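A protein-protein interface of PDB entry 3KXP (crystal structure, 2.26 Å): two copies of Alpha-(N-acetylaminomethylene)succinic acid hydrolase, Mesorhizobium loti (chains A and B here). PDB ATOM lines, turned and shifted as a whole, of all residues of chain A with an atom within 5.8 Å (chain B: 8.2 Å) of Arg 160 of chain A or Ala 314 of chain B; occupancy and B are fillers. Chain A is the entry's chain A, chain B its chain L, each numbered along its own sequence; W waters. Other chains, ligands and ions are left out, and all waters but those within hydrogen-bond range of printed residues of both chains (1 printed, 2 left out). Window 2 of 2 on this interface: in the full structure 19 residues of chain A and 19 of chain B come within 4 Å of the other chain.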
ATOM      1  N   PRO A  69     -15.084 -19.900  15.889  1.00  0.00           N
ATOM      2  CA  PRO A  69     -15.755 -19.064  16.887  1.00  0.00           C
ATOM      3  C   PRO A  69     -17.184 -19.552  17.134  1.00  0.00           C
ATOM      4  O   PRO A  69     -17.828 -20.110  16.243  1.00  0.00           O
ATOM      5  CB  PRO A  69     -15.710 -17.676  16.254  1.00  0.00           C
ATOM      6  CG  PRO A  69     -14.430 -17.716  15.477  1.00  0.00           C
ATOM      7  CD  PRO A  69     -14.499 -19.074  14.820  1.00  0.00           C
ATOM      8  N   PHE A  95     -17.540 -21.520  11.654  1.00  0.00           N
ATOM      9  CA  PHE A  95     -17.955 -21.314  13.039  1.00  0.00           C
ATOM     10  C   PHE A  95     -18.505 -22.593  13.662  1.00  0.00           C
ATOM     11  O   PHE A  95     -18.935 -23.515  12.962  1.00  0.00           O
ATOM     12  CB  PHE A  95     -19.070 -20.260  13.163  1.00  0.00           C
ATOM     13  CG  PHE A  95     -18.769 -18.942  12.507  1.00  0.00           C
ATOM     14  CD1 PHE A  95     -19.017 -18.754  11.151  1.00  0.00           C
ATOM     15  CD2 PHE A  95     -18.281 -17.877  13.254  1.00  0.00           C
ATOM     16  CE1 PHE A  95     -18.786 -17.526  10.549  1.00  0.00           C
ATOM     17  CE2 PHE A  95     -18.044 -16.642  12.659  1.00  0.00           C
ATOM     18  CZ  PHE A  95     -18.299 -16.465  11.306  1.00  0.00           C
ATOM     19  N   HIS A 135     -16.529 -15.882  23.702  1.00  0.00           N
ATOM     20  CA  HIS A 135     -17.750 -15.100  23.539  1.00  0.00           C
ATOM     21  C   HIS A 135     -18.510 -15.574  22.302  1.00  0.00           C
ATOM     22  O   HIS A 135     -17.918 -16.057  21.336  1.00  0.00           O
ATOM     23  CB  HIS A 135     -17.420 -13.603  23.443  1.00  0.00           C
ATOM     24  CG  HIS A 135     -16.508 -13.249  22.308  1.00  0.00           C
ATOM     25  ND1 HIS A 135     -16.234 -11.944  21.959  1.00  0.00           N
ATOM     26  CD2 HIS A 135     -15.834 -14.024  21.424  1.00  0.00           C
ATOM     27  CE1 HIS A 135     -15.437 -11.929  20.905  1.00  0.00           C
ATOM     28  NE2 HIS A 135     -15.180 -13.178  20.560  1.00  0.00           N
ATOM     29  N   ALA A 136     -19.828 -15.433  22.328  1.00  0.00           N
ATOM     30  CA  ALA A 136     -20.627 -15.917  21.215  1.00  0.00           C
ATOM     31  C   ALA A 136     -21.369 -14.874  20.409  1.00  0.00           C
ATOM     32  O   ALA A 136     -21.751 -13.818  20.916  1.00  0.00           O
ATOM     33  CB  ALA A 136     -21.624 -16.961  21.720  1.00  0.00           C
ATOM     34  N   ILE A 137     -21.552 -15.193  19.136  1.00  0.00           N
ATOM     35  CA  ILE A 137     -22.311 -14.364  18.223  1.00  0.00           C
ATOM     36  C   ILE A 137     -23.716 -14.940  18.368  1.00  0.00           C
ATOM     37  O   ILE A 137     -23.923 -16.138  18.173  1.00  0.00           O
ATOM     38  CB  ILE A 137     -21.822 -14.537  16.769  1.00  0.00           C
ATOM     39  CG1 ILE A 137     -20.386 -14.002  16.643  1.00  0.00           C
ATOM     40  CG2 ILE A 137     -22.777 -13.825  15.805  1.00  0.00           C
ATOM     41  CD1 ILE A 137     -19.740 -14.286  15.315  1.00  0.00           C
ATOM     42  N   PRO A 156     -22.122  -8.067  28.331  1.00  0.00           N
ATOM     43  CA  PRO A 156     -21.246  -7.540  27.282  1.00  0.00           C
ATOM     44  C   PRO A 156     -20.095  -8.463  26.903  1.00  0.00           C
ATOM     45  O   PRO A 156     -19.883  -8.759  25.727  1.00  0.00           O
ATOM     46  CB  PRO A 156     -20.737  -6.236  27.891  1.00  0.00           C
ATOM     47  CG  PRO A 156     -21.904  -5.776  28.672  1.00  0.00           C
ATOM     48  CD  PRO A 156     -22.380  -7.036  29.353  1.00  0.00           C
ATOM     49  N   ASP A 157     -19.358  -8.911  27.913  1.00  0.00           N
ATOM     50  CA  ASP A 157     -18.198  -9.774  27.716  1.00  0.00           C
ATOM     51  C   ASP A 157     -18.478 -11.160  27.130  1.00  0.00           C
ATOM     52  O   ASP A 157     -17.636 -11.725  26.432  1.00  0.00           O
ATOM     53  CB  ASP A 157     -17.446  -9.914  29.046  1.00  0.00           C
ATOM     54  CG  ASP A 157     -16.900  -8.577  29.559  1.00  0.00           C
ATOM     55  OD1 ASP A 157     -16.416  -8.531  30.710  1.00  0.00           O
ATOM     56  OD2 ASP A 157     -16.945  -7.572  28.814  1.00  0.00           O
ATOM     57  N   LEU A 158     -19.654 -11.708  27.402  1.00  0.00           N
ATOM     58  CA  LEU A 158     -19.988 -13.033  26.898  1.00  0.00           C
ATOM     59  C   LEU A 158     -20.444 -13.056  25.436  1.00  0.00           C
ATOM     60  O   LEU A 158     -20.432 -14.106  24.791  1.00  0.00           O
ATOM     61  CB  LEU A 158     -21.068 -13.660  27.788  1.00  0.00           C
ATOM     62  CG  LEU A 158     -20.674 -13.819  29.257  1.00  0.00           C
ATOM     63  CD1 LEU A 158     -21.838 -14.400  30.060  1.00  0.00           C
ATOM     64  CD2 LEU A 158     -19.444 -14.721  29.348  1.00  0.00           C
ATOM     65  N   VAL A 159     -20.842 -11.904  24.909  1.00  0.00           N
ATOM     66  CA  VAL A 159     -21.324 -11.856  23.538  1.00  0.00           C
ATOM     67  C   VAL A 159     -20.611 -10.870  22.627  1.00  0.00           C
ATOM     68  O   VAL A 159     -20.446  -9.687  22.938  1.00  0.00           O
ATOM     69  CB  VAL A 159     -22.863 -11.620  23.512  1.00  0.00           C
ATOM     70  CG1 VAL A 159     -23.277 -10.822  24.720  1.00  0.00           C
ATOM     71  CG2 VAL A 159     -23.282 -10.921  22.226  1.00  0.00           C
ATOM     72  N   ARG A 160     -20.191 -11.399  21.487  1.00  0.00           N
ATOM     73  CA  ARG A 160     -19.473 -10.657  20.464  1.00  0.00           C
ATOM     74  C   ARG A 160     -20.386  -9.740  19.647  1.00  0.00           C
ATOM     75  O   ARG A 160     -20.069  -8.572  19.422  1.00  0.00           O
ATOM     76  CB  ARG A 160     -18.770 -11.663  19.548  1.00  0.00           C
ATOM     77  CG  ARG A 160     -18.175 -11.088  18.283  1.00  0.00           C
ATOM     78  CD  ARG A 160     -17.461 -12.189  17.502  1.00  0.00           C
ATOM     79  NE  ARG A 160     -17.422 -11.893  16.072  1.00  0.00           N
ATOM     80  CZ  ARG A 160     -16.806 -12.642  15.163  1.00  0.00           C
ATOM     81  NH1 ARG A 160     -16.162 -13.745  15.525  1.00  0.00           N
ATOM     82  NH2 ARG A 160     -16.842 -12.281  13.887  1.00  0.00           N
ATOM     83  N   SER A 161     -21.522 -10.276  19.215  1.00  0.00           N
ATOM     84  CA  SER A 161     -22.464  -9.520  18.409  1.00  0.00           C
ATOM     85  C   SER A 161     -23.795 -10.246  18.305  1.00  0.00           C
ATOM     86  O   SER A 161     -23.883 -11.453  18.546  1.00  0.00           O
ATOM     87  CB  SER A 161     -21.896  -9.307  17.008  1.00  0.00           C
ATOM     88  OG  SER A 161     -21.519 -10.544  16.436  1.00  0.00           O
ATOM     89  N   VAL A 162     -24.827  -9.505  17.925  1.00  0.00           N
ATOM     90  CA  VAL A 162     -26.156 -10.071  17.797  1.00  0.00           C
ATOM     91  C   VAL A 162     -26.814  -9.770  16.463  1.00  0.00           C
ATOM     92  O   VAL A 162     -26.674  -8.677  15.919  1.00  0.00           O
ATOM     93  CB  VAL A 162     -27.102  -9.526  18.877  1.00  0.00           C
ATOM     94  CG1 VAL A 162     -28.493 -10.127  18.700  1.00  0.00           C
ATOM     95  CG2 VAL A 162     -26.549  -9.821  20.251  1.00  0.00           C
ATOM     96  N   LYS A 256     -22.659  -3.897  22.476  1.00  0.00           N
ATOM     97  CA  LYS A 256     -22.060  -4.720  21.434  1.00  0.00           C
ATOM     98  C   LYS A 256     -22.825  -4.563  20.116  1.00  0.00           C
ATOM     99  O   LYS A 256     -23.989  -4.166  20.108  1.00  0.00           O
ATOM    100  CB  LYS A 256     -22.044  -6.191  21.867  1.00  0.00           C
ATOM    101  CG  LYS A 256     -21.441  -6.421  23.245  1.00  0.00           C
ATOM    102  CD  LYS A 256     -20.097  -5.717  23.383  1.00  0.00           C
ATOM    103  CE  LYS A 256     -19.021  -6.376  22.546  1.00  0.00           C
ATOM    104  NZ  LYS A 256     -18.392  -7.497  23.287  1.00  0.00           N
ATOM    105  N   PRO A 257     -22.175  -4.877  18.983  1.00  0.00           N
ATOM    106  CA  PRO A 257     -22.800  -4.765  17.657  1.00  0.00           C
ATOM    107  C   PRO A 257     -24.108  -5.543  17.533  1.00  0.00           C
ATOM    108  O   PRO A 257     -24.188  -6.706  17.930  1.00  0.00           O
ATOM    109  CB  PRO A 257     -21.728  -5.318  16.720  1.00  0.00           C
ATOM    110  CG  PRO A 257     -20.450  -4.997  17.447  1.00  0.00           C
ATOM    111  CD  PRO A 257     -20.791  -5.366  18.867  1.00  0.00           C
ATOM    112  N   PHE A 311     -22.530  -8.780   7.773  1.00  0.00           N
ATOM    113  CA  PHE A 311     -22.400  -8.266   9.133  1.00  0.00           C
ATOM    114  C   PHE A 311     -21.122  -8.690   9.843  1.00  0.00           C
ATOM    115  O   PHE A 311     -20.274  -7.858  10.153  1.00  0.00           O
ATOM    116  CB  PHE A 311     -23.599  -8.717   9.970  1.00  0.00           C
ATOM    117  CG  PHE A 311     -23.676  -8.073  11.327  1.00  0.00           C
ATOM    118  CD1 PHE A 311     -23.994  -8.831  12.449  1.00  0.00           C
ATOM    119  CD2 PHE A 311     -23.469  -6.704  11.478  1.00  0.00           C
ATOM    120  CE1 PHE A 311     -24.109  -8.235  13.703  1.00  0.00           C
ATOM    121  CE2 PHE A 311     -23.580  -6.095  12.722  1.00  0.00           C
ATOM    122  CZ  PHE A 311     -23.903  -6.859  13.842  1.00  0.00           C
ATOM    123  N   ILE A 312     -20.989  -9.988  10.094  1.00  0.00           N
ATOM    124  CA  ILE A 312     -19.831 -10.517  10.808  1.00  0.00           C
ATOM    125  C   ILE A 312     -18.487 -10.514  10.061  1.00  0.00           C
ATOM    126  O   ILE A 312     -17.432 -10.513  10.698  1.00  0.00           O
ATOM    127  CB  ILE A 312     -20.124 -11.951  11.315  1.00  0.00           C
ATOM    128  CG1 ILE A 312     -20.484 -12.853  10.136  1.00  0.00           C
ATOM    129  CG2 ILE A 312     -21.281 -11.922  12.319  1.00  0.00           C
ATOM    130  CD1 ILE A 312     -20.801 -14.272  10.516  1.00  0.00           C
ATOM    131  N   ASP A 313     -18.516 -10.497   8.729  1.00  0.00           N
ATOM    132  CA  ASP A 313     -17.277 -10.510   7.954  1.00  0.00           C
ATOM    133  C   ASP A 313     -16.697  -9.138   7.617  1.00  0.00           C
ATOM    134  O   ASP A 313     -15.557  -9.046   7.163  1.00  0.00           O
ATOM    135  CB  ASP A 313     -17.461 -11.288   6.646  1.00  0.00           C
ATOM    136  CG  ASP A 313     -17.682 -12.772   6.871  1.00  0.00           C
ATOM    137  OD1 ASP A 313     -17.300 -13.273   7.951  1.00  0.00           O
ATOM    138  OD2 ASP A 313     -18.226 -13.435   5.957  1.00  0.00           O
ATOM    139  N   ARG B  94      -6.185   0.643  16.996  1.00  0.00           N
ATOM    140  CA  ARG B  94      -6.263  -0.742  16.519  1.00  0.00           C
ATOM    141  C   ARG B  94      -6.259  -0.903  15.011  1.00  0.00           C
ATOM    142  O   ARG B  94      -6.329  -2.022  14.489  1.00  0.00           O
ATOM    143  CB  ARG B  94      -7.487  -1.448  17.118  1.00  0.00           C
ATOM    144  CG  ARG B  94      -8.830  -0.800  16.836  1.00  0.00           C
ATOM    145  CD  ARG B  94      -9.749  -1.027  18.029  1.00  0.00           C
ATOM    146  NE  ARG B  94     -11.132  -0.652  17.763  1.00  0.00           N
ATOM    147  CZ  ARG B  94     -12.003  -1.417  17.112  1.00  0.00           C
ATOM    148  NH1 ARG B  94     -11.645  -2.611  16.656  1.00  0.00           N
ATOM    149  NH2 ARG B  94     -13.239  -0.981  16.915  1.00  0.00           N
ATOM    150  N   ARG B 160     -11.317  -5.567   2.284  1.00  0.00           N
ATOM    151  CA  ARG B 160     -12.040  -6.320   3.301  1.00  0.00           C
ATOM    152  C   ARG B 160     -13.523  -5.930   3.383  1.00  0.00           C
ATOM    153  O   ARG B 160     -14.406  -6.788   3.371  1.00  0.00           O
ATOM    154  CB  ARG B 160     -11.355  -6.104   4.652  1.00  0.00           C
ATOM    155  CG  ARG B 160     -12.183  -6.507   5.849  1.00  0.00           C
ATOM    156  CD  ARG B 160     -11.366  -6.420   7.117  1.00  0.00           C
ATOM    157  NE  ARG B 160     -12.215  -6.294   8.298  1.00  0.00           N
ATOM    158  CZ  ARG B 160     -11.750  -6.140   9.531  1.00  0.00           C
ATOM    159  NH1 ARG B 160     -10.441  -6.102   9.747  1.00  0.00           N
ATOM    160  NH2 ARG B 160     -12.590  -5.999  10.546  1.00  0.00           N
ATOM    161  N   ILE B 308     -19.570   2.752  12.400  1.00  0.00           N
ATOM    162  CA  ILE B 308     -18.421   2.094  11.791  1.00  0.00           C
ATOM    163  C   ILE B 308     -17.967   0.891  12.629  1.00  0.00           C
ATOM    164  O   ILE B 308     -17.735  -0.198  12.092  1.00  0.00           O
ATOM    165  CB  ILE B 308     -17.244   3.087  11.613  1.00  0.00           C
ATOM    166  CG1 ILE B 308     -17.610   4.118  10.540  1.00  0.00           C
ATOM    167  CG2 ILE B 308     -15.965   2.341  11.233  1.00  0.00           C
ATOM    168  CD1 ILE B 308     -16.595   5.226  10.367  1.00  0.00           C
ATOM    169  N   THR B 309     -17.862   1.077  13.941  1.00  0.00           N
ATOM    170  CA  THR B 309     -17.424  -0.009  14.804  1.00  0.00           C
ATOM    171  C   THR B 309     -18.443  -1.149  14.923  1.00  0.00           C
ATOM    172  O   THR B 309     -18.051  -2.305  15.053  1.00  0.00           O
ATOM    173  CB  THR B 309     -17.039   0.504  16.215  1.00  0.00           C
ATOM    174  OG1 THR B 309     -18.178   1.079  16.859  1.00  0.00           O
ATOM    175  CG2 THR B 309     -15.952   1.559  16.113  1.00  0.00           C
ATOM    176  N   ASN B 310     -19.739  -0.848  14.875  1.00  0.00           N
ATOM    177  CA  ASN B 310     -20.726  -1.920  14.964  1.00  0.00           C
ATOM    178  C   ASN B 310     -20.569  -2.838  13.759  1.00  0.00           C
ATOM    179  O   ASN B 310     -20.767  -4.052  13.849  1.00  0.00           O
ATOM    180  CB  ASN B 310     -22.160  -1.371  14.978  1.00  0.00           C
ATOM    181  CG  ASN B 310     -22.517  -0.700  16.287  1.00  0.00           C
ATOM    182  OD1 ASN B 310     -22.099  -1.140  17.357  1.00  0.00           O
ATOM    183  ND2 ASN B 310     -23.309   0.362  16.212  1.00  0.00           N
ATOM    184  N   PHE B 311     -20.203  -2.232  12.637  1.00  0.00           N
ATOM    185  CA  PHE B 311     -20.027  -2.921  11.366  1.00  0.00           C
ATOM    186  C   PHE B 311     -18.764  -3.791  11.291  1.00  0.00           C
ATOM    187  O   PHE B 311     -18.841  -4.982  10.996  1.00  0.00           O
ATOM    188  CB  PHE B 311     -20.013  -1.872  10.244  1.00  0.00           C
ATOM    189  CG  PHE B 311     -19.904  -2.440   8.862  1.00  0.00           C
ATOM    190  CD1 PHE B 311     -18.897  -2.009   8.003  1.00  0.00           C
ATOM    191  CD2 PHE B 311     -20.828  -3.367   8.395  1.00  0.00           C
ATOM    192  CE1 PHE B 311     -18.816  -2.495   6.693  1.00  0.00           C
ATOM    193  CE2 PHE B 311     -20.757  -3.856   7.090  1.00  0.00           C
ATOM    194  CZ  PHE B 311     -19.749  -3.417   6.239  1.00  0.00           C
ATOM    195  N   ILE B 312     -17.602  -3.199  11.554  1.00  0.00           N
ATOM    196  CA  ILE B 312     -16.348  -3.945  11.474  1.00  0.00           C
ATOM    197  C   ILE B 312     -16.048  -4.868  12.659  1.00  0.00           C
ATOM    198  O   ILE B 312     -15.277  -5.815  12.513  1.00  0.00           O
ATOM    199  CB  ILE B 312     -15.150  -2.992  11.272  1.00  0.00           C
ATOM    200  CG1 ILE B 312     -15.094  -1.982  12.419  1.00  0.00           C
ATOM    201  CG2 ILE B 312     -15.277  -2.270   9.929  1.00  0.00           C
ATOM    202  CD1 ILE B 312     -13.946  -0.984  12.317  1.00  0.00           C
ATOM    203  N   ASP B 313     -16.653  -4.602  13.820  1.00  0.00           N
ATOM    204  CA  ASP B 313     -16.427  -5.427  15.014  1.00  0.00           C
ATOM    205  C   ASP B 313     -17.461  -6.534  15.227  1.00  0.00           C
ATOM    206  O   ASP B 313     -17.375  -7.282  16.207  1.00  0.00           O
ATOM    207  CB  ASP B 313     -16.396  -4.565  16.287  1.00  0.00           C
ATOM    208  CG  ASP B 313     -15.251  -3.555  16.296  1.00  0.00           C
ATOM    209  OD1 ASP B 313     -14.196  -3.823  15.681  1.00  0.00           O
ATOM    210  OD2 ASP B 313     -15.404  -2.495  16.939  1.00  0.00           O
ATOM    211  N   ALA B 314     -18.431  -6.649  14.324  1.00  0.00           N
ATOM    212  CA  ALA B 314     -19.473  -7.667  14.463  1.00  0.00           C
ATOM    213  C   ALA B 314     -18.902  -9.085  14.529  1.00  0.00           C
ATOM    214  O   ALA B 314     -17.957  -9.420  13.809  1.00  0.00           O
ATOM    215  CB  ALA B 314     -20.483  -7.553  13.313  1.00  0.00           C
HETATM  216  O   HOH W   1     -23.522  -1.198  19.939  1.00  0.00           O
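The backbone carbonyl oxygen of Ala 314 of chain B lies within hydrogen-bond range of the guanidinium group of Arg 160 of chain A, 3.1 Å away.
The backbone carbonyl oxygen (O) of Phe 311 of chain A sits close to the backbone carbonyl oxygen (O) of Phe 311 of chain B, 3.3 Å away.
The backbone carbonyl oxygen (O) of Ala 314 of chain B lies close to the backbone carbonyl oxygen (O) of Ile 312 of chain A, 3.3 Å away.
The backbone carbonyl oxygen of Ala 136 of chain A lies within hydrogen-bond range of the backbone NH of Arg 160 of chain A, 2.9 Å away.
The backbone NH (N) of Val 162 of chain A is in hydrogen-bond range of the backbone carbonyl oxygen (O) of Pro 257 of chain A (2.9 Å).
Ala 314 of chain B touches Ser 161 of chain A.
CB of Pro 257 of chain A touches O of Asn 310 of chain B, at 3.3 Å.
CB of Pro 257 of chain A touches CA of Ala 314 of chain B, at 3.96 Å.
Asn 310 of chain B touches Phe 311 of chain A (O to CE2, 3.7 Å).
CB of Ala 314 of chain B touches O of Phe 311 of chain A, 3.2 Å away.
Ala 136 of chain A touches none of the printed residues of chain B.
Of chain B, only Ala 314 (3.1 Å) comes within 4 Å of Arg 160 of chain A.
Ser 161 of chain A touches one residue of chain B.
Printed residues of chain B within 4 Å of Ile 312 of chain A: Ala 314 (3.3 Å).
Printed residues of chain A within 4 Å of Asn 310 of chain B: Pro 257 (3.3 Å) and Phe 311 (3.7 Å).
Ile 312 of chain B touches none of the printed residues of chain A.
Ala 314 of chain B touches just these residues of chain A: Arg 160, Ser 161, Pro 257, Phe 311 and Ile 312.
The nearest printed residue of chain A that does not touch Phe 311 of chain B is Pro 257 of chain A (5.3 Å).
Of the 17 printed residues of chain A, 5 touch a printed residue of chain B.
Printed residues of chain A that touch a printed residue of chain B: Arg 160, Ser 161, Pro 257, Phe 311 and Ile 312.
Of the 9 printed residues of chain B, 3 touch a printed residue of chain A.
Printed residues of chain B that touch a printed residue of chain A: Asn 310, Phe 311 and Ala 314.
Among the printed residues, no Asp or Glu carboxylate lies within 4 Å of a Lys or Arg side-chain nitrogen of the other chain.
Phe 311 of chain A touches its own counterpart, Phe 311 of chain B.
4 positions are printed for both chains.
Of the 8 pairs that touch across the chains among the printed residues, 1 has its exchanged pair printed and touching as well.
Water W1 bridges OD1 of Asn 310 of chain B and O of Lys 256 of chain A.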
